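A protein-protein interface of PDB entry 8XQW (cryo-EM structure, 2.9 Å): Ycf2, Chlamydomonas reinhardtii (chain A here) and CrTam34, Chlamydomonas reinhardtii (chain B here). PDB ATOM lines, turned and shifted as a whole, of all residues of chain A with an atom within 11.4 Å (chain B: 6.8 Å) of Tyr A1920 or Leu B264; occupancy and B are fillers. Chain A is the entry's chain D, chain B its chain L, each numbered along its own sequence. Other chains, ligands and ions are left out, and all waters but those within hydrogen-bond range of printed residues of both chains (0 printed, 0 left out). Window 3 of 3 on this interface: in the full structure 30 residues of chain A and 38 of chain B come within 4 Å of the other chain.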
ATOM      1  N   LEU A 319      -5.597  23.371   7.334  1.00  0.00           N
ATOM      2  CA  LEU A 319      -5.759  21.970   7.672  1.00  0.00           C
ATOM      3  C   LEU A 319      -5.340  21.084   6.505  1.00  0.00           C
ATOM      4  O   LEU A 319      -5.107  21.544   5.391  1.00  0.00           O
ATOM      5  CB  LEU A 319      -7.202  21.680   8.061  1.00  0.00           C
ATOM      6  CG  LEU A 319      -7.418  21.338   9.523  1.00  0.00           C
ATOM      7  CD1 LEU A 319      -7.354  22.591  10.341  1.00  0.00           C
ATOM      8  CD2 LEU A 319      -8.737  20.640   9.704  1.00  0.00           C
ATOM      9  N   PHE A 321      -6.268  17.321   4.301  1.00  0.00           N
ATOM     10  CA  PHE A 321      -7.454  16.712   3.703  1.00  0.00           C
ATOM     11  C   PHE A 321      -7.638  15.326   4.307  1.00  0.00           C
ATOM     12  O   PHE A 321      -7.252  14.306   3.738  1.00  0.00           O
ATOM     13  CB  PHE A 321      -7.298  16.647   2.193  1.00  0.00           C
ATOM     14  CG  PHE A 321      -8.589  16.542   1.447  1.00  0.00           C
ATOM     15  CD1 PHE A 321      -9.585  17.477   1.622  1.00  0.00           C
ATOM     16  CD2 PHE A 321      -8.790  15.522   0.542  1.00  0.00           C
ATOM     17  CE1 PHE A 321     -10.758  17.381   0.921  1.00  0.00           C
ATOM     18  CE2 PHE A 321      -9.960  15.428  -0.157  1.00  0.00           C
ATOM     19  CZ  PHE A 321     -10.944  16.357   0.032  1.00  0.00           C
ATOM     20  N   VAL A 322      -8.243  15.290   5.488  1.00  0.00           N
ATOM     21  CA  VAL A 322      -8.371  14.056   6.248  1.00  0.00           C
ATOM     22  C   VAL A 322      -9.750  13.997   6.888  1.00  0.00           C
ATOM     23  O   VAL A 322     -10.368  15.024   7.175  1.00  0.00           O
ATOM     24  CB  VAL A 322      -7.264  13.932   7.316  1.00  0.00           C
ATOM     25  CG1 VAL A 322      -5.929  13.721   6.665  1.00  0.00           C
ATOM     26  CG2 VAL A 322      -7.215  15.164   8.170  1.00  0.00           C
ATOM     27  N   PHE A 323     -10.233  12.778   7.102  1.00  0.00           N
ATOM     28  CA  PHE A 323     -11.504  12.571   7.772  1.00  0.00           C
ATOM     29  C   PHE A 323     -11.406  12.974   9.234  1.00  0.00           C
ATOM     30  O   PHE A 323     -10.328  13.250   9.757  1.00  0.00           O
ATOM     31  CB  PHE A 323     -11.921  11.110   7.700  1.00  0.00           C
ATOM     32  CG  PHE A 323     -12.346  10.652   6.346  1.00  0.00           C
ATOM     33  CD1 PHE A 323     -13.627  10.866   5.902  1.00  0.00           C
ATOM     34  CD2 PHE A 323     -11.480   9.957   5.539  1.00  0.00           C
ATOM     35  CE1 PHE A 323     -14.022  10.423   4.680  1.00  0.00           C
ATOM     36  CE2 PHE A 323     -11.872   9.521   4.310  1.00  0.00           C
ATOM     37  CZ  PHE A 323     -13.144   9.749   3.884  1.00  0.00           C
ATOM     38  N   THR A 324     -12.548  12.986   9.904  1.00  0.00           N
ATOM     39  CA  THR A 324     -12.590  13.188  11.342  1.00  0.00           C
ATOM     40  C   THR A 324     -12.970  11.875  12.022  1.00  0.00           C
ATOM     41  O   THR A 324     -13.365  10.909  11.372  1.00  0.00           O
ATOM     42  CB  THR A 324     -13.541  14.321  11.695  1.00  0.00           C
ATOM     43  OG1 THR A 324     -14.548  14.422  10.685  1.00  0.00           O
ATOM     44  CG2 THR A 324     -12.799  15.622  11.796  1.00  0.00           C
ATOM     45  N   LEU A 326     -15.255  10.398  14.176  1.00  0.00           N
ATOM     46  CA  LEU A 326     -16.576   9.818  13.931  1.00  0.00           C
ATOM     47  C   LEU A 326     -17.019   8.796  14.972  1.00  0.00           C
ATOM     48  O   LEU A 326     -18.165   8.349  14.937  1.00  0.00           O
ATOM     49  CB  LEU A 326     -16.616   9.181  12.541  1.00  0.00           C
ATOM     50  CG  LEU A 326     -17.928   8.709  11.942  1.00  0.00           C
ATOM     51  CD1 LEU A 326     -18.335   9.683  10.889  1.00  0.00           C
ATOM     52  CD2 LEU A 326     -17.749   7.345  11.352  1.00  0.00           C
ATOM     53  N   LYS A 329     -18.064  10.131  20.012  1.00  0.00           N
ATOM     54  CA  LYS A 329     -19.326  10.417  20.674  1.00  0.00           C
ATOM     55  C   LYS A 329     -20.099   9.155  21.024  1.00  0.00           C
ATOM     56  O   LYS A 329     -20.417   8.928  22.190  1.00  0.00           O
ATOM     57  CB  LYS A 329     -20.172  11.317  19.778  1.00  0.00           C
ATOM     58  CG  LYS A 329     -20.984  12.344  20.504  1.00  0.00           C
ATOM     59  CD  LYS A 329     -21.101  13.595  19.673  1.00  0.00           C
ATOM     60  CE  LYS A 329     -22.306  14.415  20.075  1.00  0.00           C
ATOM     61  NZ  LYS A 329     -22.285  14.761  21.518  1.00  0.00           N
ATOM     62  N   ASN A1915     -33.417  20.455  18.718  1.00  0.00           N
ATOM     63  CA  ASN A1915     -32.579  21.597  18.385  1.00  0.00           C
ATOM     64  C   ASN A1915     -31.141  21.360  18.808  1.00  0.00           C
ATOM     65  O   ASN A1915     -30.548  22.166  19.522  1.00  0.00           O
ATOM     66  CB  ASN A1915     -33.118  22.864  19.040  1.00  0.00           C
ATOM     67  CG  ASN A1915     -34.006  23.654  18.115  1.00  0.00           C
ATOM     68  OD1 ASN A1915     -35.054  24.158  18.514  1.00  0.00           O
ATOM     69  ND2 ASN A1915     -33.596  23.759  16.859  1.00  0.00           N
ATOM     70  N   LYS A1916     -30.590  20.231  18.365  1.00  0.00           N
ATOM     71  CA  LYS A1916     -29.208  19.898  18.677  1.00  0.00           C
ATOM     72  C   LYS A1916     -28.275  20.195  17.517  1.00  0.00           C
ATOM     73  O   LYS A1916     -27.055  20.138  17.686  1.00  0.00           O
ATOM     74  CB  LYS A1916     -29.105  18.420  19.050  1.00  0.00           C
ATOM     75  CG  LYS A1916     -29.789  18.056  20.353  1.00  0.00           C
ATOM     76  CD  LYS A1916     -29.322  16.701  20.849  1.00  0.00           C
ATOM     77  CE  LYS A1916     -29.801  16.440  22.259  1.00  0.00           C
ATOM     78  NZ  LYS A1916     -29.143  15.239  22.826  1.00  0.00           N
ATOM     79  N   ILE A1917     -28.823  20.513  16.346  1.00  0.00           N
ATOM     80  CA  ILE A1917     -28.064  20.551  15.106  1.00  0.00           C
ATOM     81  C   ILE A1917     -28.242  21.855  14.347  1.00  0.00           C
ATOM     82  O   ILE A1917     -27.586  22.055  13.321  1.00  0.00           O
ATOM     83  CB  ILE A1917     -28.434  19.352  14.208  1.00  0.00           C
ATOM     84  CG1 ILE A1917     -27.294  19.014  13.246  1.00  0.00           C
ATOM     85  CG2 ILE A1917     -29.740  19.619  13.483  1.00  0.00           C
ATOM     86  CD1 ILE A1917     -27.435  17.666  12.619  1.00  0.00           C
ATOM     87  N   LYS A1918     -29.094  22.753  14.823  1.00  0.00           N
ATOM     88  CA  LYS A1918     -29.330  24.039  14.176  1.00  0.00           C
ATOM     89  C   LYS A1918     -28.086  24.930  14.153  1.00  0.00           C
ATOM     90  O   LYS A1918     -27.794  25.534  13.111  1.00  0.00           O
ATOM     91  CB  LYS A1918     -30.484  24.765  14.865  1.00  0.00           C
ATOM     92  CG  LYS A1918     -31.459  25.430  13.914  1.00  0.00           C
ATOM     93  CD  LYS A1918     -32.678  25.957  14.660  1.00  0.00           C
ATOM     94  CE  LYS A1918     -33.699  26.561  13.710  1.00  0.00           C
ATOM     95  NZ  LYS A1918     -35.053  26.656  14.327  1.00  0.00           N
ATOM     96  N   PRO A1919     -27.332  25.056  15.255  1.00  0.00           N
ATOM     97  CA  PRO A1919     -26.174  25.964  15.237  1.00  0.00           C
ATOM     98  C   PRO A1919     -25.182  25.694  14.122  1.00  0.00           C
ATOM     99  O   PRO A1919     -24.585  26.644  13.603  1.00  0.00           O
ATOM    100  CB  PRO A1919     -25.533  25.742  16.615  1.00  0.00           C
ATOM    101  CG  PRO A1919     -26.140  24.496  17.136  1.00  0.00           C
ATOM    102  CD  PRO A1919     -27.516  24.487  16.599  1.00  0.00           C
ATOM    103  N   TYR A1920     -24.993  24.435  13.726  1.00  0.00           N
ATOM    104  CA  TYR A1920     -24.049  24.142  12.655  1.00  0.00           C
ATOM    105  C   TYR A1920     -24.516  24.672  11.309  1.00  0.00           C
ATOM    106  O   TYR A1920     -23.704  24.778  10.388  1.00  0.00           O
ATOM    107  CB  TYR A1920     -23.804  22.642  12.555  1.00  0.00           C
ATOM    108  CG  TYR A1920     -23.277  22.015  13.817  1.00  0.00           C
ATOM    109  CD1 TYR A1920     -21.918  21.953  14.070  1.00  0.00           C
ATOM    110  CD2 TYR A1920     -24.139  21.474  14.753  1.00  0.00           C
ATOM    111  CE1 TYR A1920     -21.438  21.376  15.220  1.00  0.00           C
ATOM    112  CE2 TYR A1920     -23.668  20.896  15.902  1.00  0.00           C
ATOM    113  CZ  TYR A1920     -22.319  20.847  16.131  1.00  0.00           C
ATOM    114  OH  TYR A1920     -21.852  20.268  17.285  1.00  0.00           O
ATOM    115  N   PHE A1921     -25.800  24.992  11.167  1.00  0.00           N
ATOM    116  CA  PHE A1921     -26.292  25.612   9.945  1.00  0.00           C
ATOM    117  C   PHE A1921     -26.420  27.122  10.080  1.00  0.00           C
ATOM    118  O   PHE A1921     -26.248  27.851   9.090  1.00  0.00           O
ATOM    119  CB  PHE A1921     -27.639  25.001   9.560  1.00  0.00           C
ATOM    120  CG  PHE A1921     -27.558  23.546   9.196  1.00  0.00           C
ATOM    121  CD1 PHE A1921     -27.624  22.572  10.170  1.00  0.00           C
ATOM    122  CD2 PHE A1921     -27.410  23.155   7.880  1.00  0.00           C
ATOM    123  CE1 PHE A1921     -27.551  21.238   9.840  1.00  0.00           C
ATOM    124  CE2 PHE A1921     -27.334  21.823   7.547  1.00  0.00           C
ATOM    125  CZ  PHE A1921     -27.403  20.864   8.528  1.00  0.00           C
ATOM    126  N   GLU A1922     -26.719  27.603  11.290  1.00  0.00           N
ATOM    127  CA  GLU A1922     -26.696  29.042  11.529  1.00  0.00           C
ATOM    128  C   GLU A1922     -25.288  29.595  11.381  1.00  0.00           C
ATOM    129  O   GLU A1922     -25.107  30.765  11.026  1.00  0.00           O
ATOM    130  CB  GLU A1922     -27.248  29.370  12.915  1.00  0.00           C
ATOM    131  CG  GLU A1922     -28.669  29.903  12.913  1.00  0.00           C
ATOM    132  CD  GLU A1922     -29.699  28.812  12.755  1.00  0.00           C
ATOM    133  OE1 GLU A1922     -29.417  27.674  13.173  1.00  0.00           O
ATOM    134  OE2 GLU A1922     -30.795  29.089  12.230  1.00  0.00           O
ATOM    135  N   ALA A1923     -24.275  28.770  11.641  1.00  0.00           N
ATOM    136  CA  ALA A1923     -22.901  29.220  11.460  1.00  0.00           C
ATOM    137  C   ALA A1923     -22.593  29.518  10.000  1.00  0.00           C
ATOM    138  O   ALA A1923     -21.530  30.065   9.689  1.00  0.00           O
ATOM    139  CB  ALA A1923     -21.926  28.174  12.001  1.00  0.00           C
ATOM    140  N   TYR A1924     -23.498  29.165   9.091  1.00  0.00           N
ATOM    141  CA  TYR A1924     -23.274  29.394   7.672  1.00  0.00           C
ATOM    142  C   TYR A1924     -24.281  30.357   7.060  1.00  0.00           C
ATOM    143  O   TYR A1924     -23.882  31.311   6.389  1.00  0.00           O
ATOM    144  CB  TYR A1924     -23.286  28.062   6.916  1.00  0.00           C
ATOM    145  CG  TYR A1924     -21.983  27.315   7.026  1.00  0.00           C
ATOM    146  CD1 TYR A1924     -21.646  26.644   8.190  1.00  0.00           C
ATOM    147  CD2 TYR A1924     -21.083  27.294   5.976  1.00  0.00           C
ATOM    148  CE1 TYR A1924     -20.457  25.970   8.303  1.00  0.00           C
ATOM    149  CE2 TYR A1924     -19.889  26.619   6.080  1.00  0.00           C
ATOM    150  CZ  TYR A1924     -19.582  25.960   7.249  1.00  0.00           C
ATOM    151  OH  TYR A1924     -18.393  25.285   7.368  1.00  0.00           O
ATOM    152  N   PHE A1925     -25.582  30.153   7.272  1.00  0.00           N
ATOM    153  CA  PHE A1925     -26.486  31.096   6.620  1.00  0.00           C
ATOM    154  C   PHE A1925     -26.738  32.350   7.445  1.00  0.00           C
ATOM    155  O   PHE A1925     -27.758  33.015   7.232  1.00  0.00           O
ATOM    156  CB  PHE A1925     -27.820  30.435   6.230  1.00  0.00           C
ATOM    157  CG  PHE A1925     -28.538  29.743   7.350  1.00  0.00           C
ATOM    158  CD1 PHE A1925     -28.918  30.423   8.493  1.00  0.00           C
ATOM    159  CD2 PHE A1925     -28.881  28.414   7.231  1.00  0.00           C
ATOM    160  CE1 PHE A1925     -29.593  29.780   9.502  1.00  0.00           C
ATOM    161  CE2 PHE A1925     -29.555  27.764   8.238  1.00  0.00           C
ATOM    162  CZ  PHE A1925     -29.912  28.447   9.373  1.00  0.00           C
ATOM    163  N   SER A1926     -25.841  32.689   8.364  1.00  0.00           N
ATOM    164  CA  SER A1926     -25.945  33.924   9.136  1.00  0.00           C
ATOM    165  C   SER A1926     -25.511  35.134   8.311  1.00  0.00           C
ATOM    166  O   SER A1926     -24.719  35.012   7.375  1.00  0.00           O
ATOM    167  CB  SER A1926     -25.105  33.830  10.409  1.00  0.00           C
ATOM    168  OG  SER A1926     -23.774  34.253  10.176  1.00  0.00           O
ATOM    169  N   LEU B 254     -26.215  13.514   5.970  1.00  0.00           N
ATOM    170  CA  LEU B 254     -25.656  14.809   6.337  1.00  0.00           C
ATOM    171  C   LEU B 254     -25.912  15.115   7.804  1.00  0.00           C
ATOM    172  O   LEU B 254     -24.995  15.489   8.541  1.00  0.00           O
ATOM    173  CB  LEU B 254     -26.246  15.901   5.456  1.00  0.00           C
ATOM    174  CG  LEU B 254     -25.334  16.411   4.356  1.00  0.00           C
ATOM    175  CD1 LEU B 254     -26.064  17.412   3.503  1.00  0.00           C
ATOM    176  CD2 LEU B 254     -24.145  17.044   4.984  1.00  0.00           C
ATOM    177  N   ALA B 255     -27.155  14.950   8.248  1.00  0.00           N
ATOM    178  CA  ALA B 255     -27.476  15.216   9.642  1.00  0.00           C
ATOM    179  C   ALA B 255     -26.726  14.277  10.572  1.00  0.00           C
ATOM    180  O   ALA B 255     -26.158  14.714  11.579  1.00  0.00           O
ATOM    181  CB  ALA B 255     -28.977  15.089   9.861  1.00  0.00           C
ATOM    182  N   LEU B 257     -23.943  12.541  10.087  1.00  0.00           N
ATOM    183  CA  LEU B 257     -22.515  12.819  10.087  1.00  0.00           C
ATOM    184  C   LEU B 257     -22.204  14.094  10.847  1.00  0.00           C
ATOM    185  O   LEU B 257     -21.203  14.164  11.563  1.00  0.00           O
ATOM    186  CB  LEU B 257     -22.002  12.934   8.657  1.00  0.00           C
ATOM    187  CG  LEU B 257     -21.770  11.643   7.894  1.00  0.00           C
ATOM    188  CD1 LEU B 257     -21.147  11.962   6.573  1.00  0.00           C
ATOM    189  CD2 LEU B 257     -20.866  10.764   8.683  1.00  0.00           C
ATOM    190  N   THR B 258     -23.038  15.122  10.697  1.00  0.00           N
ATOM    191  CA  THR B 258     -22.819  16.343  11.458  1.00  0.00           C
ATOM    192  C   THR B 258     -22.910  16.076  12.947  1.00  0.00           C
ATOM    193  O   THR B 258     -22.138  16.630  13.732  1.00  0.00           O
ATOM    194  CB  THR B 258     -23.835  17.397  11.058  1.00  0.00           C
ATOM    195  OG1 THR B 258     -23.806  17.567   9.637  1.00  0.00           O
ATOM    196  CG2 THR B 258     -23.511  18.704  11.725  1.00  0.00           C
ATOM    197  N   TRP B 259     -23.848  15.229  13.357  1.00  0.00           N
ATOM    198  CA  TRP B 259     -23.989  14.951  14.778  1.00  0.00           C
ATOM    199  C   TRP B 259     -22.835  14.105  15.297  1.00  0.00           C
ATOM    200  O   TRP B 259     -22.356  14.321  16.414  1.00  0.00           O
ATOM    201  CB  TRP B 259     -25.317  14.260  15.046  1.00  0.00           C
ATOM    202  CG  TRP B 259     -25.375  13.653  16.382  1.00  0.00           C
ATOM    203  CD1 TRP B 259     -25.158  14.275  17.561  1.00  0.00           C
ATOM    204  CD2 TRP B 259     -25.662  12.292  16.689  1.00  0.00           C
ATOM    205  NE1 TRP B 259     -25.292  13.390  18.593  1.00  0.00           N
ATOM    206  CE2 TRP B 259     -25.603  12.161  18.079  1.00  0.00           C
ATOM    207  CE3 TRP B 259     -25.965  11.171  15.919  1.00  0.00           C
ATOM    208  CZ2 TRP B 259     -25.837  10.959  18.720  1.00  0.00           C
ATOM    209  CZ3 TRP B 259     -26.196   9.977  16.558  1.00  0.00           C
ATOM    210  CH2 TRP B 259     -26.131   9.879  17.942  1.00  0.00           C
ATOM    211  N   SER B 261     -19.562  13.505  13.844  1.00  0.00           N
ATOM    212  CA  SER B 261     -18.225  14.063  13.722  1.00  0.00           C
ATOM    213  C   SER B 261     -18.092  15.427  14.367  1.00  0.00           C
ATOM    214  O   SER B 261     -16.970  15.861  14.631  1.00  0.00           O
ATOM    215  CB  SER B 261     -17.823  14.162  12.255  1.00  0.00           C
ATOM    216  OG  SER B 261     -18.851  14.761  11.498  1.00  0.00           O
ATOM    217  N   GLY B 262     -19.195  16.112  14.621  1.00  0.00           N
ATOM    218  CA  GLY B 262     -19.146  17.385  15.291  1.00  0.00           C
ATOM    219  C   GLY B 262     -18.895  18.578  14.402  1.00  0.00           C
ATOM    220  O   GLY B 262     -18.747  19.688  14.920  1.00  0.00           O
ATOM    221  N   ARG B 263     -18.843  18.400  13.087  1.00  0.00           N
ATOM    222  CA  ARG B 263     -18.636  19.534  12.204  1.00  0.00           C
ATOM    223  C   ARG B 263     -19.329  19.282  10.876  1.00  0.00           C
ATOM    224  O   ARG B 263     -19.301  18.173  10.346  1.00  0.00           O
ATOM    225  CB  ARG B 263     -17.148  19.814  11.993  1.00  0.00           C
ATOM    226  CG  ARG B 263     -16.374  18.710  11.317  1.00  0.00           C
ATOM    227  CD  ARG B 263     -16.019  19.093   9.898  1.00  0.00           C
ATOM    228  NE  ARG B 263     -14.920  18.297   9.373  1.00  0.00           N
ATOM    229  CZ  ARG B 263     -13.671  18.734   9.259  1.00  0.00           C
ATOM    230  NH1 ARG B 263     -13.365  19.970   9.627  1.00  0.00           N
ATOM    231  NH2 ARG B 263     -12.729  17.940   8.767  1.00  0.00           N
ATOM    232  N   LEU B 264     -19.940  20.326  10.348  1.00  0.00           N
ATOM    233  CA  LEU B 264     -20.700  20.215   9.113  1.00  0.00           C
ATOM    234  C   LEU B 264     -19.760  19.993   7.935  1.00  0.00           C
ATOM    235  O   LEU B 264     -18.797  20.745   7.773  1.00  0.00           O
ATOM    236  CB  LEU B 264     -21.521  21.466   8.876  1.00  0.00           C
ATOM    237  CG  LEU B 264     -22.599  21.278   7.820  1.00  0.00           C
ATOM    238  CD1 LEU B 264     -23.811  20.634   8.437  1.00  0.00           C
ATOM    239  CD2 LEU B 264     -22.965  22.595   7.188  1.00  0.00           C
ATOM    240  N   PRO B 265     -20.007  18.989   7.096  1.00  0.00           N
ATOM    241  CA  PRO B 265     -19.102  18.716   5.972  1.00  0.00           C
ATOM    242  C   PRO B 265     -19.317  19.702   4.836  1.00  0.00           C
ATOM    243  O   PRO B 265     -20.426  19.851   4.326  1.00  0.00           O
ATOM    244  CB  PRO B 265     -19.474  17.292   5.559  1.00  0.00           C
ATOM    245  CG  PRO B 265     -20.856  17.123   6.015  1.00  0.00           C
ATOM    246  CD  PRO B 265     -21.032  17.945   7.243  1.00  0.00           C
ATOM    247  N   THR B 266     -18.242  20.359   4.434  1.00  0.00           N
ATOM    248  CA  THR B 266     -18.236  21.348   3.367  1.00  0.00           C
ATOM    249  C   THR B 266     -17.335  20.849   2.245  1.00  0.00           C
ATOM    250  O   THR B 266     -16.605  19.872   2.443  1.00  0.00           O
ATOM    251  CB  THR B 266     -17.751  22.687   3.908  1.00  0.00           C
ATOM    252  OG1 THR B 266     -16.344  22.615   4.162  1.00  0.00           O
ATOM    253  CG2 THR B 266     -18.467  23.012   5.196  1.00  0.00           C
ATOM    254  N   THR B 269     -13.825  19.156   2.792  1.00  0.00           N
ATOM    255  CA  THR B 269     -13.619  17.957   3.578  1.00  0.00           C
ATOM    256  C   THR B 269     -13.980  16.713   2.778  1.00  0.00           C
ATOM    257  O   THR B 269     -14.884  16.754   1.942  1.00  0.00           O
ATOM    258  CB  THR B 269     -14.475  18.013   4.839  1.00  0.00           C
ATOM    259  OG1 THR B 269     -15.844  18.142   4.461  1.00  0.00           O
ATOM    260  CG2 THR B 269     -14.086  19.209   5.666  1.00  0.00           C
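The side-chain hydroxyl (OG1) of Thr B258 is in hydrogen-bond range of the backbone carbonyl oxygen (O) of Leu B254. The side-chain hydroxyl of Ser B261 lies within hydrogen-bond range of the backbone carbonyl oxygen of Leu B257, at 2.4 Å. OG1 of Thr B269 sits at hydrogen-bond distance from O of Thr B266, 2.8 Å away.
Among the printed residues, merely in contact across the chains: Tyr A1924 with Thr B266, Tyr A1920 with Gly B262, Ile A1917 with Ala B255, Lys A329 with Trp B259, Leu A326 with Leu B257, Phe A1921 with Leu B264, Thr A324 with Ser B261, Phe A321 with Thr B269, Thr A324 with Arg B263, Tyr A1920 with Thr B258, Ile A1917 with Thr B258 and Tyr A1920 with Leu B264.
Tyr A1920 touches just these residues of chain B: Thr B258, Gly B262 and Leu B264. Leu B264 touches just these residues of chain A: Tyr A1920 (3.9 Å) and Phe A1921 (3.6 Å). Thr B258 touches just these residues of chain A: Ile A1917 and Tyr A1920. Of chain A, only Tyr A1920 comes within 4 Å of Gly B262. Thr B266 touches one residue of chain A. Of the printed residues of chain B, Lys A329 touches Trp B259. Printed residues of chain B within 4 Å of Phe A321: Thr B269 (3.8 Å). Printed residues of chain A within 4 Å of Ser B261: Thr A324 (3.6 Å). Of the printed residues of chain B, Phe A1921 touches Leu B264. Of the printed residues of chain B, Thr A324 touches Ser B261 and Arg B263. The nearest printed residue of chain B that does not touch Lys A329 is Gly B262 (6.0 Å).
Of the 12 printed residues of chain B, 10 touch a printed residue of chain A. Of the 19 printed residues of chain A, 8 touch a printed residue of chain B. Printed residues of chain A that touch a printed residue of chain B: Phe A321, Thr A324, Leu A326, Lys A329, Ile A1917, Tyr A1920, Phe A1921 and Tyr A1924. Among the printed residues, 12 pairs touch across the chains. Among the printed residues, no Asp or Glu carboxylate lies within 4 Å of a Lys or Arg side-chain nitrogen of the other chain.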
